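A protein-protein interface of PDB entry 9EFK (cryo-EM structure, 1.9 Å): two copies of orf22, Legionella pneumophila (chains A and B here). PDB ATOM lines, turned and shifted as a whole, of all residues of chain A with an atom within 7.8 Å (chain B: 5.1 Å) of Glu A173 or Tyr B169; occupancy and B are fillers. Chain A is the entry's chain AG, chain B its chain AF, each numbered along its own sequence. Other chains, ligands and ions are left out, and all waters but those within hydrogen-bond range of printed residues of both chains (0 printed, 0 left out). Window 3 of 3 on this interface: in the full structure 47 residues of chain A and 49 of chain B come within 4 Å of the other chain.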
ATOM      1  N   GLY A 154      11.608  15.747   5.087  1.00  0.00           N
ATOM      2  CA  GLY A 154      12.793  14.981   4.770  1.00  0.00           C
ATOM      3  C   GLY A 154      14.027  15.789   4.452  1.00  0.00           C
ATOM      4  O   GLY A 154      14.940  15.270   3.812  1.00  0.00           O
ATOM      5  N   VAL A 156      17.321  18.573   5.437  1.00  0.00           N
ATOM      6  CA  VAL A 156      18.295  18.964   6.443  1.00  0.00           C
ATOM      7  C   VAL A 156      18.844  20.336   6.068  1.00  0.00           C
ATOM      8  O   VAL A 156      18.596  20.852   4.981  1.00  0.00           O
ATOM      9  CB  VAL A 156      19.436  17.940   6.582  1.00  0.00           C
ATOM     10  CG1 VAL A 156      18.879  16.567   6.875  1.00  0.00           C
ATOM     11  CG2 VAL A 156      20.276  17.911   5.322  1.00  0.00           C
ATOM     12  N   THR A 170      17.261  17.982   0.448  1.00  0.00           N
ATOM     13  CA  THR A 170      16.562  16.710   0.570  1.00  0.00           C
ATOM     14  C   THR A 170      17.563  15.565   0.525  1.00  0.00           C
ATOM     15  O   THR A 170      18.376  15.476  -0.399  1.00  0.00           O
ATOM     16  CB  THR A 170      15.534  16.543  -0.547  1.00  0.00           C
ATOM     17  OG1 THR A 170      14.670  17.682  -0.583  1.00  0.00           O
ATOM     18  CG2 THR A 170      14.702  15.301  -0.312  1.00  0.00           C
ATOM     19  N   ILE A 171      17.502  14.691   1.521  1.00  0.00           N
ATOM     20  CA  ILE A 171      18.380  13.531   1.588  1.00  0.00           C
ATOM     21  C   ILE A 171      17.699  12.370   0.877  1.00  0.00           C
ATOM     22  O   ILE A 171      16.572  11.995   1.220  1.00  0.00           O
ATOM     23  CB  ILE A 171      18.720  13.173   3.040  1.00  0.00           C
ATOM     24  CG1 ILE A 171      19.786  14.126   3.574  1.00  0.00           C
ATOM     25  CG2 ILE A 171      19.187  11.733   3.142  1.00  0.00           C
ATOM     26  CD1 ILE A 171      20.340  13.725   4.908  1.00  0.00           C
ATOM     27  N   ASP A 172      18.387  11.797  -0.116  1.00  0.00           N
ATOM     28  CA  ASP A 172      17.784  10.752  -0.938  1.00  0.00           C
ATOM     29  C   ASP A 172      17.451   9.504  -0.130  1.00  0.00           C
ATOM     30  O   ASP A 172      16.540   8.755  -0.501  1.00  0.00           O
ATOM     31  CB  ASP A 172      18.703  10.404  -2.115  1.00  0.00           C
ATOM     32  CG  ASP A 172      20.089   9.946  -1.679  1.00  0.00           C
ATOM     33  OD1 ASP A 172      20.418  10.022  -0.477  1.00  0.00           O
ATOM     34  OD2 ASP A 172      20.862   9.505  -2.555  1.00  0.00           O
ATOM     35  N   GLU A 173      18.164   9.268   0.969  1.00  0.00           N
ATOM     36  CA  GLU A 173      17.890   8.148   1.865  1.00  0.00           C
ATOM     37  C   GLU A 173      17.939   6.797   1.152  1.00  0.00           C
ATOM     38  O   GLU A 173      18.643   6.631   0.156  1.00  0.00           O
ATOM     39  CB  GLU A 173      16.527   8.333   2.539  1.00  0.00           C
ATOM     40  CG  GLU A 173      16.166   7.239   3.524  1.00  0.00           C
ATOM     41  CD  GLU A 173      14.839   7.493   4.213  1.00  0.00           C
ATOM     42  OE1 GLU A 173      14.034   8.286   3.682  1.00  0.00           O
ATOM     43  OE2 GLU A 173      14.602   6.902   5.288  1.00  0.00           O
ATOM     44  N   GLY B 154      26.572   9.895  15.042  1.00  0.00           N
ATOM     45  CA  GLY B 154      26.361   9.825  13.609  1.00  0.00           C
ATOM     46  C   GLY B 154      24.978  10.222  13.143  1.00  0.00           C
ATOM     47  O   GLY B 154      24.466   9.641  12.181  1.00  0.00           O
ATOM     48  N   GLN B 155      24.365  11.213  13.783  1.00  0.00           N
ATOM     49  CA  GLN B 155      23.016  11.631  13.440  1.00  0.00           C
ATOM     50  C   GLN B 155      22.984  13.114  13.092  1.00  0.00           C
ATOM     51  O   GLN B 155      23.838  13.895  13.517  1.00  0.00           O
ATOM     52  CB  GLN B 155      22.035  11.337  14.579  1.00  0.00           C
ATOM     53  CG  GLN B 155      21.825   9.860  14.837  1.00  0.00           C
ATOM     54  CD  GLN B 155      20.608   9.579  15.690  1.00  0.00           C
ATOM     55  OE1 GLN B 155      20.456  10.127  16.775  1.00  0.00           O
ATOM     56  NE2 GLN B 155      19.729   8.719  15.197  1.00  0.00           N
ATOM     57  N   VAL B 156      21.981  13.486  12.295  1.00  0.00           N
ATOM     58  CA  VAL B 156      21.751  14.858  11.868  1.00  0.00           C
ATOM     59  C   VAL B 156      20.300  15.211  12.159  1.00  0.00           C
ATOM     60  O   VAL B 156      19.457  14.340  12.375  1.00  0.00           O
ATOM     61  CB  VAL B 156      22.060  15.069  10.370  1.00  0.00           C
ATOM     62  CG1 VAL B 156      23.480  14.663  10.052  1.00  0.00           C
ATOM     63  CG2 VAL B 156      21.080  14.295   9.512  1.00  0.00           C
ATOM     64  N   ARG B 158      16.782  16.319  10.923  1.00  0.00           N
ATOM     65  CA  ARG B 158      16.057  16.154   9.672  1.00  0.00           C
ATOM     66  C   ARG B 158      14.566  16.218   9.951  1.00  0.00           C
ATOM     67  O   ARG B 158      14.067  15.487  10.809  1.00  0.00           O
ATOM     68  CB  ARG B 158      16.431  14.825   9.015  1.00  0.00           C
ATOM     69  CG  ARG B 158      15.671  14.485   7.755  1.00  0.00           C
ATOM     70  CD  ARG B 158      16.106  13.126   7.254  1.00  0.00           C
ATOM     71  NE  ARG B 158      15.380  12.700   6.066  1.00  0.00           N
ATOM     72  CZ  ARG B 158      14.286  11.954   6.087  1.00  0.00           C
ATOM     73  NH1 ARG B 158      13.749  11.548   7.225  1.00  0.00           N
ATOM     74  NH2 ARG B 158      13.717  11.605   4.938  1.00  0.00           N
ATOM     75  N   ASP B 161       9.171  12.780   7.634  1.00  0.00           N
ATOM     76  CA  ASP B 161       8.447  12.659   6.372  1.00  0.00           C
ATOM     77  C   ASP B 161       7.086  13.340   6.426  1.00  0.00           C
ATOM     78  O   ASP B 161       6.604  13.839   5.405  1.00  0.00           O
ATOM     79  CB  ASP B 161       8.281  11.187   6.004  1.00  0.00           C
ATOM     80  CG  ASP B 161       9.606  10.482   5.817  1.00  0.00           C
ATOM     81  OD1 ASP B 161      10.563  11.127   5.342  1.00  0.00           O
ATOM     82  OD2 ASP B 161       9.691   9.282   6.147  1.00  0.00           O
ATOM     83  N   GLU B 167      13.557  15.390  13.692  1.00  0.00           N
ATOM     84  CA  GLU B 167      13.962  14.162  14.353  1.00  0.00           C
ATOM     85  C   GLU B 167      15.415  13.852  14.022  1.00  0.00           C
ATOM     86  O   GLU B 167      15.959  14.313  13.019  1.00  0.00           O
ATOM     87  CB  GLU B 167      13.055  12.993  13.955  1.00  0.00           C
ATOM     88  CG  GLU B 167      12.672  12.969  12.487  1.00  0.00           C
ATOM     89  CD  GLU B 167      13.700  12.279  11.613  1.00  0.00           C
ATOM     90  OE1 GLU B 167      14.402  11.378  12.119  1.00  0.00           O
ATOM     91  OE2 GLU B 167      13.805  12.633  10.421  1.00  0.00           O
ATOM     92  N   ALA B 168      16.047  13.078  14.901  1.00  0.00           N
ATOM     93  CA  ALA B 168      17.422  12.650  14.692  1.00  0.00           C
ATOM     94  C   ALA B 168      17.468  11.528  13.663  1.00  0.00           C
ATOM     95  O   ALA B 168      16.729  10.547  13.768  1.00  0.00           O
ATOM     96  CB  ALA B 168      18.043  12.192  16.009  1.00  0.00           C
ATOM     97  N   TYR B 169      18.341  11.675  12.672  1.00  0.00           N
ATOM     98  CA  TYR B 169      18.414  10.770  11.533  1.00  0.00           C
ATOM     99  C   TYR B 169      19.857  10.333  11.336  1.00  0.00           C
ATOM    100  O   TYR B 169      20.757  11.174  11.279  1.00  0.00           O
ATOM    101  CB  TYR B 169      17.871  11.461  10.281  1.00  0.00           C
ATOM    102  CG  TYR B 169      18.012  10.680   9.002  1.00  0.00           C
ATOM    103  CD1 TYR B 169      17.075   9.728   8.640  1.00  0.00           C
ATOM    104  CD2 TYR B 169      19.068  10.920   8.140  1.00  0.00           C
ATOM    105  CE1 TYR B 169      17.196   9.023   7.466  1.00  0.00           C
ATOM    106  CE2 TYR B 169      19.199  10.221   6.966  1.00  0.00           C
ATOM    107  CZ  TYR B 169      18.261   9.274   6.633  1.00  0.00           C
ATOM    108  OH  TYR B 169      18.391   8.574   5.457  1.00  0.00           O
ATOM    109  N   THR B 170      20.075   9.026  11.214  1.00  0.00           N
ATOM    110  CA  THR B 170      21.421   8.465  11.180  1.00  0.00           C
ATOM    111  C   THR B 170      21.973   8.454   9.760  1.00  0.00           C
ATOM    112  O   THR B 170      21.285   8.046   8.821  1.00  0.00           O
ATOM    113  CB  THR B 170      21.425   7.048  11.752  1.00  0.00           C
ATOM    114  OG1 THR B 170      20.887   7.065  13.077  1.00  0.00           O
ATOM    115  CG2 THR B 170      22.837   6.503  11.808  1.00  0.00           C
ATOM    116  N   ILE B 171      23.216   8.905   9.613  1.00  0.00           N
ATOM    117  CA  ILE B 171      23.950   8.856   8.354  1.00  0.00           C
ATOM    118  C   ILE B 171      25.258   8.116   8.594  1.00  0.00           C
ATOM    119  O   ILE B 171      26.018   8.475   9.500  1.00  0.00           O
ATOM    120  CB  ILE B 171      24.222  10.264   7.797  1.00  0.00           C
ATOM    121  CG1 ILE B 171      22.919  10.942   7.383  1.00  0.00           C
ATOM    122  CG2 ILE B 171      25.190  10.201   6.630  1.00  0.00           C
ATOM    123  CD1 ILE B 171      23.117  12.331   6.852  1.00  0.00           C
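Arg B158 touches Val A156.
Ile A171 touches Tyr B169 (CG2 to OH, 3.997 Å).
Ile B171 touches Ile A171.
OH of Tyr B169 touches CG of Glu A173, 3.2 Å away.
Glu A173 touches two residues of chain B.
Printed residues of chain A within 4 Å of Tyr B169: Ile A171 (3.997 Å) and Glu A173 (3.2 Å).
No residue of chain A comes within 4 Å of Ala B168.
Printed residues of chain B within 4 Å of Gly A154: Arg B158 (3.4 Å).
Printed residues of chain B within 4 Å of Val A156: Arg B158 (3.7 Å).
Of the printed residues of chain A, Arg B158 touches Gly A154 (3.4 Å), Val A156 (3.7 Å) and Glu A173 (3.6 Å).
Printed residues of chain A within 4 Å of Ile B171: Ile A171.
The nearest printed residue of chain A that does not touch Tyr B169 is Asp A172 (5.7 Å).
Hydrophobic or aromatic side chains of chain B within 4 Å of the printed part of chain A: Tyr B169 and Ile B171.
Hydrophobic or aromatic side chains of chain A within 4 Å of the printed part of chain B: Val A156 and Ile A171.
Among the printed residues, 6 pairs touch across the chains.
Among the printed residues, Asp or Glu carboxylates within 4 Å of a Lys or Arg side-chain nitrogen of the other chain: Glu A173 with Arg B158 (3.6 Å).
The backbone NH (N) of Ile B171 sits at hydrogen-bond distance from the backbone carbonyl oxygen (O) of Gly B154.
The backbone NH (N) of Val B156 lies within hydrogen-bond range of the backbone carbonyl oxygen (O) of Tyr B169 (2.8 Å).
The side-chain carboxylate of Asp B161 is in salt-bridge range of the guanidinium group of Arg B158 (3.2 Å).
OE2 of Glu B167 lies within salt-bridge range of NH1 of Arg B158.
The backbone NH (N) of Ile A171 sits at hydrogen-bond distance from the backbone carbonyl oxygen (O) of Gly A154 (3.5 Å).
The guanidinium group (NE) of Arg B158 sits at hydrogen-bond distance from the backbone carbonyl oxygen (O) of Gly A154, 3.4 Å away.
The side-chain carboxylate (OE1) of Glu A173 is in salt-bridge range of the guanidinium group (NH2) of Arg B158.
Ile A171 touches its own counterpart, Ile B171.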
